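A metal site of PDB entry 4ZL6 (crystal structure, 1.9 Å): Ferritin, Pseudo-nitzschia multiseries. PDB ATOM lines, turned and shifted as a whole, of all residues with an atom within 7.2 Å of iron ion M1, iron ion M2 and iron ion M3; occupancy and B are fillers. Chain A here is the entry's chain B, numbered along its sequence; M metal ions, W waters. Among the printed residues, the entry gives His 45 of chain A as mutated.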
ATOM      1  N   GLN A  12      32.463 -22.810 -12.687  1.00  0.00           N
ATOM      2  CA  GLN A  12      32.246 -23.085 -11.292  1.00  0.00           C
ATOM      3  C   GLN A  12      32.514 -21.857 -10.439  1.00  0.00           C
ATOM      4  O   GLN A  12      31.814 -21.631  -9.452  1.00  0.00           O
ATOM      5  CB  GLN A  12      33.129 -24.239 -10.825  1.00  0.00           C
ATOM      6  CG  GLN A  12      32.810 -24.739  -9.441  1.00  0.00           C
ATOM      7  CD  GLN A  12      31.413 -25.324  -9.423  1.00  0.00           C
ATOM      8  OE1 GLN A  12      30.930 -25.939 -10.411  1.00  0.00           O
ATOM      9  NE2 GLN A  12      30.731 -25.097  -8.346  1.00  0.00           N
ATOM     10  N   GLN A  15      29.503 -19.857 -10.701  1.00  0.00           N
ATOM     11  CA  GLN A  15      28.440 -20.455  -9.922  1.00  0.00           C
ATOM     12  C   GLN A  15      28.553 -20.079  -8.437  1.00  0.00           C
ATOM     13  O   GLN A  15      27.533 -19.781  -7.831  1.00  0.00           O
ATOM     14  CB  GLN A  15      28.283 -21.990 -10.109  1.00  0.00           C
ATOM     15  CG  GLN A  15      27.658 -22.330 -11.461  1.00  0.00           C
ATOM     16  CD  GLN A  15      26.377 -21.532 -11.654  1.00  0.00           C
ATOM     17  OE1 GLN A  15      25.432 -21.744 -10.888  1.00  0.00           O
ATOM     18  NE2 GLN A  15      26.412 -20.466 -12.555  1.00  0.00           N
ATOM     19  N   GLU A  16      29.772 -20.149  -7.869  1.00  0.00           N
ATOM     20  CA  GLU A  16      29.963 -19.827  -6.456  1.00  0.00           C
ATOM     21  C   GLU A  16      29.678 -18.351  -6.149  1.00  0.00           C
ATOM     22  O   GLU A  16      28.977 -18.066  -5.174  1.00  0.00           O
ATOM     23  CB  GLU A  16      31.377 -20.119  -6.049  1.00  0.00           C
ATOM     24  CG  GLU A  16      31.817 -21.549  -6.132  1.00  0.00           C
ATOM     25  CD  GLU A  16      30.956 -22.532  -5.351  1.00  0.00           C
ATOM     26  OE1 GLU A  16      30.353 -22.175  -4.316  1.00  0.00           O
ATOM     27  OE2 GLU A  16      30.934 -23.696  -5.782  1.00  0.00           O
ATOM     28  N   ALA A  19      25.937 -17.872  -6.389  1.00  0.00           N
ATOM     29  CA  ALA A  19      25.317 -18.338  -5.153  1.00  0.00           C
ATOM     30  C   ALA A  19      25.586 -17.356  -4.023  1.00  0.00           C
ATOM     31  O   ALA A  19      24.683 -17.073  -3.219  1.00  0.00           O
ATOM     32  CB  ALA A  19      25.793 -19.767  -4.788  1.00  0.00           C
ATOM     33  N   SER A  20      26.782 -16.737  -3.981  1.00  0.00           N
ATOM     34  CA  SER A  20      27.015 -15.759  -2.948  1.00  0.00           C
ATOM     35  C   SER A  20      25.985 -14.597  -2.970  1.00  0.00           C
ATOM     36  O   SER A  20      25.448 -14.147  -1.908  1.00  0.00           O
ATOM     37  CB  SER A  20      28.464 -15.242  -3.079  1.00  0.00           C
ATOM     38  OG  SER A  20      28.694 -14.328  -2.103  1.00  0.00           O
ATOM     39  N   TYR A  23      22.434 -15.821  -1.844  1.00  0.00           N
ATOM     40  CA  TYR A  23      22.395 -15.856  -0.386  1.00  0.00           C
ATOM     41  C   TYR A  23      22.271 -14.448   0.184  1.00  0.00           C
ATOM     42  O   TYR A  23      21.479 -14.222   1.131  1.00  0.00           O
ATOM     43  CB  TYR A  23      23.636 -16.570   0.211  1.00  0.00           C
ATOM     44  CG  TYR A  23      23.512 -18.052   0.332  1.00  0.00           C
ATOM     45  CD1 TYR A  23      22.737 -18.623   1.332  1.00  0.00           C
ATOM     46  CD2 TYR A  23      24.173 -18.895  -0.536  1.00  0.00           C
ATOM     47  CE1 TYR A  23      22.618 -20.002   1.496  1.00  0.00           C
ATOM     48  CE2 TYR A  23      23.993 -20.275  -0.435  1.00  0.00           C
ATOM     49  CZ  TYR A  23      23.277 -20.803   0.597  1.00  0.00           C
ATOM     50  OH  TYR A  23      23.196 -22.132   0.733  1.00  0.00           O
ATOM     51  N   TYR A  41      22.098 -16.171   9.131  1.00  0.00           N
ATOM     52  CA  TYR A  41      22.544 -17.407   8.551  1.00  0.00           C
ATOM     53  C   TYR A  41      22.833 -17.219   7.025  1.00  0.00           C
ATOM     54  O   TYR A  41      23.860 -17.661   6.493  1.00  0.00           O
ATOM     55  CB  TYR A  41      21.510 -18.494   8.738  1.00  0.00           C
ATOM     56  CG  TYR A  41      21.803 -19.730   7.997  1.00  0.00           C
ATOM     57  CD1 TYR A  41      21.425 -19.846   6.674  1.00  0.00           C
ATOM     58  CD2 TYR A  41      22.508 -20.765   8.581  1.00  0.00           C
ATOM     59  CE1 TYR A  41      21.734 -20.950   5.944  1.00  0.00           C
ATOM     60  CE2 TYR A  41      22.810 -21.910   7.853  1.00  0.00           C
ATOM     61  CZ  TYR A  41      22.430 -21.997   6.553  1.00  0.00           C
ATOM     62  OH  TYR A  41      22.740 -23.062   5.784  1.00  0.00           O
ATOM     63  N   HIS A  45      26.459 -17.607   5.016  1.00  0.00           N
ATOM     64  CA  HIS A  45      26.600 -18.559   3.963  1.00  0.00           C
ATOM     65  C   HIS A  45      27.011 -17.786   2.659  1.00  0.00           C
ATOM     66  O   HIS A  45      27.768 -18.292   1.871  1.00  0.00           O
ATOM     67  CB  HIS A  45      25.308 -19.330   3.765  1.00  0.00           C
ATOM     68  CG  HIS A  45      25.520 -20.665   3.146  1.00  0.00           C
ATOM     69  ND1 HIS A  45      25.034 -21.827   3.711  1.00  0.00           N
ATOM     70  CD2 HIS A  45      26.272 -21.046   2.070  1.00  0.00           C
ATOM     71  CE1 HIS A  45      25.373 -22.852   2.939  1.00  0.00           C
ATOM     72  NE2 HIS A  45      26.177 -22.407   1.979  1.00  0.00           N
ATOM     73  N   GLU A  48      30.685 -17.549   2.799  1.00  0.00           N
ATOM     74  CA  GLU A  48      31.243 -18.856   2.578  1.00  0.00           C
ATOM     75  C   GLU A  48      31.241 -19.248   1.091  1.00  0.00           C
ATOM     76  O   GLU A  48      32.217 -19.857   0.593  1.00  0.00           O
ATOM     77  CB  GLU A  48      30.421 -19.915   3.361  1.00  0.00           C
ATOM     78  CG  GLU A  48      30.893 -21.304   2.972  1.00  0.00           C
ATOM     79  CD  GLU A  48      30.367 -22.403   3.891  1.00  0.00           C
ATOM     80  OE1 GLU A  48      29.116 -22.543   4.025  1.00  0.00           O
ATOM     81  OE2 GLU A  48      31.222 -23.140   4.431  1.00  0.00           O
ATOM     82  N   GLU A  49      30.164 -18.912   0.371  1.00  0.00           N
ATOM     83  CA  GLU A  49      30.174 -19.230  -1.059  1.00  0.00           C
ATOM     84  C   GLU A  49      31.291 -18.430  -1.781  1.00  0.00           C
ATOM     85  O   GLU A  49      31.923 -18.885  -2.704  1.00  0.00           O
ATOM     86  CB  GLU A  49      28.895 -18.819  -1.724  1.00  0.00           C
ATOM     87  CG  GLU A  49      27.729 -19.541  -1.196  1.00  0.00           C
ATOM     88  CD  GLU A  49      27.753 -21.033  -1.496  1.00  0.00           C
ATOM     89  OE1 GLU A  49      28.447 -21.576  -2.333  1.00  0.00           O
ATOM     90  OE2 GLU A  49      26.925 -21.637  -0.949  1.00  0.00           O
ATOM     91  N   ARG A  50      31.443 -17.185  -1.372  1.00  0.00           N
ATOM     92  CA  ARG A  50      32.515 -16.364  -1.935  1.00  0.00           C
ATOM     93  C   ARG A  50      33.855 -17.024  -1.655  1.00  0.00           C
ATOM     94  O   ARG A  50      34.728 -17.103  -2.544  1.00  0.00           O
ATOM     95  CB  ARG A  50      32.515 -14.957  -1.379  1.00  0.00           C
ATOM     96  CG  ARG A  50      33.532 -14.053  -2.094  1.00  0.00           C
ATOM     97  CD  ARG A  50      33.243 -12.552  -1.973  1.00  0.00           C
ATOM     98  NE  ARG A  50      34.390 -11.754  -2.447  1.00  0.00           N
ATOM     99  CZ  ARG A  50      35.511 -11.616  -1.716  1.00  0.00           C
ATOM    100  NH1 ARG A  50      35.654 -12.153  -0.532  1.00  0.00           N
ATOM    101  NH2 ARG A  50      36.530 -11.008  -2.226  1.00  0.00           N
ATOM    102  N   HIS A  52      34.524 -20.234  -1.314  1.00  0.00           N
ATOM    103  CA  HIS A  52      34.617 -21.297  -2.274  1.00  0.00           C
ATOM    104  C   HIS A  52      35.064 -20.841  -3.641  1.00  0.00           C
ATOM    105  O   HIS A  52      35.990 -21.449  -4.255  1.00  0.00           O
ATOM    106  CB  HIS A  52      33.317 -22.060  -2.478  1.00  0.00           C
ATOM    107  CG  HIS A  52      32.797 -22.680  -1.239  1.00  0.00           C
ATOM    108  ND1 HIS A  52      33.619 -23.001  -0.183  1.00  0.00           N
ATOM    109  CD2 HIS A  52      31.529 -23.021  -0.878  1.00  0.00           C
ATOM    110  CE1 HIS A  52      32.882 -23.520   0.790  1.00  0.00           C
ATOM    111  NE2 HIS A  52      31.628 -23.555   0.390  1.00  0.00           N
ATOM    112  N   GLY A  53      34.450 -19.785  -4.160  1.00  0.00           N
ATOM    113  CA  GLY A  53      34.941 -19.295  -5.405  1.00  0.00           C
ATOM    114  C   GLY A  53      36.414 -18.879  -5.379  1.00  0.00           C
ATOM    115  O   GLY A  53      37.159 -19.148  -6.305  1.00  0.00           O
ATOM    116  N   PHE A  56      38.611 -21.904  -5.712  1.00  0.00           N
ATOM    117  CA  PHE A  56      38.728 -22.333  -7.083  1.00  0.00           C
ATOM    118  C   PHE A  56      39.683 -21.458  -7.826  1.00  0.00           C
ATOM    119  O   PHE A  56      40.484 -21.966  -8.641  1.00  0.00           O
ATOM    120  CB  PHE A  56      37.392 -22.385  -7.759  1.00  0.00           C
ATOM    121  CG  PHE A  56      36.626 -23.689  -7.458  1.00  0.00           C
ATOM    122  CD1 PHE A  56      36.037 -23.902  -6.230  1.00  0.00           C
ATOM    123  CD2 PHE A  56      36.607 -24.724  -8.361  1.00  0.00           C
ATOM    124  CE1 PHE A  56      35.407 -25.091  -5.893  1.00  0.00           C
ATOM    125  CE2 PHE A  56      35.953 -25.929  -8.040  1.00  0.00           C
ATOM    126  CZ  PHE A  56      35.380 -26.109  -6.807  1.00  0.00           C
ATOM    127  N   LEU A  94      19.352 -23.946  -5.142  1.00  0.00           N
ATOM    128  CA  LEU A  94      20.627 -23.330  -5.485  1.00  0.00           C
ATOM    129  C   LEU A  94      21.732 -24.313  -5.129  1.00  0.00           C
ATOM    130  O   LEU A  94      22.693 -24.525  -5.879  1.00  0.00           O
ATOM    131  CB  LEU A  94      20.728 -22.030  -4.665  1.00  0.00           C
ATOM    132  CG  LEU A  94      22.023 -21.240  -4.778  1.00  0.00           C
ATOM    133  CD1 LEU A  94      22.134 -20.601  -6.136  1.00  0.00           C
ATOM    134  CD2 LEU A  94      22.162 -20.232  -3.681  1.00  0.00           C
ATOM    135  N   GLU A  95      21.668 -24.887  -3.930  1.00  0.00           N
ATOM    136  CA  GLU A  95      22.657 -25.877  -3.552  1.00  0.00           C
ATOM    137  C   GLU A  95      22.617 -27.137  -4.373  1.00  0.00           C
ATOM    138  O   GLU A  95      23.667 -27.701  -4.716  1.00  0.00           O
ATOM    139  CB  GLU A  95      22.615 -26.164  -2.052  1.00  0.00           C
ATOM    140  CG  GLU A  95      23.086 -25.001  -1.175  1.00  0.00           C
ATOM    141  CD  GLU A  95      24.561 -24.684  -1.237  1.00  0.00           C
ATOM    142  OE1 GLU A  95      25.327 -25.403  -1.911  1.00  0.00           O
ATOM    143  OE2 GLU A  95      24.972 -23.696  -0.572  1.00  0.00           O
ATOM    144  N   ASN A  98      24.476 -26.172  -7.368  1.00  0.00           N
ATOM    145  CA  ASN A  98      25.913 -26.076  -7.064  1.00  0.00           C
ATOM    146  C   ASN A  98      26.461 -27.569  -7.131  1.00  0.00           C
ATOM    147  O   ASN A  98      27.502 -27.849  -7.712  1.00  0.00           O
ATOM    148  CB  ASN A  98      26.268 -25.481  -5.644  1.00  0.00           C
ATOM    149  CG  ASN A  98      26.060 -23.922  -5.417  1.00  0.00           C
ATOM    150  OD1 ASN A  98      25.895 -23.123  -6.344  1.00  0.00           O
ATOM    151  ND2 ASN A  98      26.129 -23.483  -4.107  1.00  0.00           N
ATOM    152  N   LEU A 102      29.338 -29.172  -9.661  1.00  0.00           N
ATOM    153  CA  LEU A 102      30.593 -29.801  -9.175  1.00  0.00           C
ATOM    154  C   LEU A 102      30.779 -31.161  -9.749  1.00  0.00           C
ATOM    155  O   LEU A 102      31.912 -31.599 -10.061  1.00  0.00           O
ATOM    156  CB  LEU A 102      30.614 -29.923  -7.656  1.00  0.00           C
ATOM    157  CG  LEU A 102      31.020 -28.698  -6.904  1.00  0.00           C
ATOM    158  CD1 LEU A 102      30.773 -29.014  -5.423  1.00  0.00           C
ATOM    159  CD2 LEU A 102      32.483 -28.358  -7.131  1.00  0.00           C
ATOM    160  N   PHE A 124      35.047 -30.648  -1.494  1.00  0.00           N
ATOM    161  CA  PHE A 124      33.855 -29.952  -1.910  1.00  0.00           C
ATOM    162  C   PHE A 124      32.697 -30.946  -2.167  1.00  0.00           C
ATOM    163  O   PHE A 124      31.528 -30.600  -1.904  1.00  0.00           O
ATOM    164  CB  PHE A 124      34.118 -29.176  -3.198  1.00  0.00           C
ATOM    165  CG  PHE A 124      35.106 -28.058  -3.032  1.00  0.00           C
ATOM    166  CD1 PHE A 124      34.668 -26.829  -2.551  1.00  0.00           C
ATOM    167  CD2 PHE A 124      36.471 -28.229  -3.316  1.00  0.00           C
ATOM    168  CE1 PHE A 124      35.589 -25.784  -2.362  1.00  0.00           C
ATOM    169  CE2 PHE A 124      37.410 -27.191  -3.116  1.00  0.00           C
ATOM    170  CZ  PHE A 124      36.961 -25.991  -2.627  1.00  0.00           C
ATOM    171  N   GLN A 127      31.476 -31.566   1.390  1.00  0.00           N
ATOM    172  CA  GLN A 127      30.812 -30.386   1.908  1.00  0.00           C
ATOM    173  C   GLN A 127      29.400 -30.231   1.313  1.00  0.00           C
ATOM    174  O   GLN A 127      28.472 -29.895   2.084  1.00  0.00           O
ATOM    175  CB  GLN A 127      31.621 -29.105   1.612  1.00  0.00           C
ATOM    176  CG  GLN A 127      30.846 -27.818   2.003  1.00  0.00           C
ATOM    177  CD  GLN A 127      31.729 -26.643   2.496  1.00  0.00           C
ATOM    178  OE1 GLN A 127      31.193 -25.592   2.890  1.00  0.00           O
ATOM    179  NE2 GLN A 127      33.067 -26.810   2.467  1.00  0.00           N
ATOM    180  N   GLN A 128      29.247 -30.424   0.016  1.00  0.00           N
ATOM    181  CA  GLN A 128      27.930 -30.291  -0.621  1.00  0.00           C
ATOM    182  C   GLN A 128      26.939 -31.286   0.002  1.00  0.00           C
ATOM    183  O   GLN A 128      25.766 -30.945   0.196  1.00  0.00           O
ATOM    184  CB  GLN A 128      27.948 -30.449  -2.137  1.00  0.00           C
ATOM    185  CG  GLN A 128      28.541 -29.260  -2.841  1.00  0.00           C
ATOM    186  CD  GLN A 128      27.804 -27.991  -2.462  1.00  0.00           C
ATOM    187  OE1 GLN A 128      28.313 -27.145  -1.707  1.00  0.00           O
ATOM    188  NE2 GLN A 128      26.536 -27.925  -2.852  1.00  0.00           N
ATOM    189  N   GLU A 131      25.881 -29.719   3.295  1.00  0.00           N
ATOM    190  CA  GLU A 131      25.046 -28.517   3.098  1.00  0.00           C
ATOM    191  C   GLU A 131      23.658 -28.824   2.644  1.00  0.00           C
ATOM    192  O   GLU A 131      22.719 -28.241   3.192  1.00  0.00           O
ATOM    193  CB  GLU A 131      25.712 -27.550   2.108  1.00  0.00           C
ATOM    194  CG  GLU A 131      26.868 -26.909   2.812  1.00  0.00           C
ATOM    195  CD  GLU A 131      27.526 -25.840   1.976  1.00  0.00           C
ATOM    196  OE1 GLU A 131      26.868 -25.392   1.045  1.00  0.00           O
ATOM    197  OE2 GLU A 131      28.683 -25.517   2.274  1.00  0.00           O
ATOM    198  N   ILE A 135      20.414 -27.835   4.843  1.00  0.00           N
ATOM    199  CA  ILE A 135      19.422 -26.919   4.274  1.00  0.00           C
ATOM    200  C   ILE A 135      18.083 -27.636   4.208  1.00  0.00           C
ATOM    201  O   ILE A 135      17.049 -27.088   4.624  1.00  0.00           O
ATOM    202  CB  ILE A 135      19.799 -26.425   2.883  1.00  0.00           C
ATOM    203  CG1 ILE A 135      21.097 -25.600   2.944  1.00  0.00           C
ATOM    204  CG2 ILE A 135      18.655 -25.617   2.290  1.00  0.00           C
ATOM    205  CD1 ILE A 135      20.992 -24.299   3.683  1.00  0.00           C
HETATM  206 FE    FE M   1      27.037 -23.487   0.082  1.00  0.00          FE
HETATM  207 FE    FE M   2      30.168 -24.722   1.145  1.00  0.00          FE
HETATM  208 FE    FE M   3      29.336 -23.320  -2.836  1.00  0.00          FE
HETATM  209  O   HOH W   1      27.895 -24.635  -1.603  1.00  0.00           O
HETATM  210  O   HOH W   2      28.790 -22.995   1.064  1.00  0.00           O
HETATM  211  O   HOH W   3      30.393 -25.231  -3.581  1.00  0.00           O
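Merely in contact with iron ion M3: Asn 98.
Within 4 Å of iron ion M3: Glu 16, Glu 49, His 52 and Asn 98.
Iron ion M1 is bound by water W2 (2.1 Å), OE2 of Glu 49 (2.1 Å), OE1 of Glu 131 (2.1 Å), OE2 of Glu 95 (2.2 Å), water W1 (2.2 Å) and NE2 of His 45 (2.3 Å).
Iron ion M1 has six donor atoms within binding distance.
Water W1 lies within hydrogen-bond range of the side-chain amide oxygen (OE1) of Gln 128 (2.5 Å), the side-chain carboxylate (OE1) of Glu 95 (2.7 Å) and the side-chain amide nitrogen (ND2) of Asn 98 (3.3 Å).
Water W3 lies within hydrogen-bond range of the side-chain carboxylate (OE2) of Glu 16 (2.7 Å) and the side-chain amide oxygen (OE1) of Gln 128 (3.4 Å).
Of the 23 residues printed, 4 come within 4 Å of iron ion M1.
The nearest printed residue that does not touch iron ion M1 is Tyr 23 (4.1 Å).
NE2 of His 52 is bound to iron ion M2 (2.0 Å).
Iron ion M2 is bound by OE2 of Glu 131, at 2.0 Å.
Iron ion M2 is bound by OE1 of Gln 127 (2.2 Å).
Iron ion M2 is bound by water W2, 2.2 Å away.
Merely in contact with iron ion M2: Glu 48 (3.6 Å).
Four residues have an atom within 4 Å of iron ion M2: Glu 48, His 52, Gln 127 and Glu 131.
Along chain A the residues within 4 Å of iron ion M2 span positions 48 to 131.
The nearest printed residue that does not touch iron ion M2 is Gln 128 (4.2 Å).
The side-chain carboxylate (OE2) of Glu 16 lies within hydrogen-bond range of the side-chain amide nitrogen (NE2) of Gln 12 (2.9 Å).
The side-chain carboxylate (OE2) of Glu 95 lies close to the side-chain hydroxyl (OH) of Tyr 23, 2.7 Å away.
The side-chain carboxylate (OE1) of Glu 49 sits close to the side-chain amide nitrogen (ND2) of Asn 98.
A ring nitrogen (ND1) of His 45 sits at hydrogen-bond distance from the side-chain hydroxyl (OH) of Tyr 41 (3.3 Å).
The side-chain carboxylate (OE1) of Glu 95 sits at hydrogen-bond distance from the side-chain amide nitrogen (ND2) of Asn 98.
The side-chain amide oxygen (OE1) of Gln 127 lies close to the side-chain carboxylate (OE2) of Glu 48 (2.9 Å).
OE1 of Glu 95 lies within hydrogen-bond range of NE2 of Gln 128, 3.0 Å away.
A ring nitrogen (NE2) of His 45 lies close to the side-chain hydroxyl of Tyr 23 (3.2 Å).
Iron ion M3 is bound by OE1 of Glu 49 (2.0 Å).
OE1 of Glu 16 is bound to iron ion M3, at 2.1 Å.
Iron ion M3 is bound by water W3 (2.3 Å).
Iron ion M3 is bound by water W1, 2.3 Å away.
Iron ion M3 has four donor atoms within binding distance.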
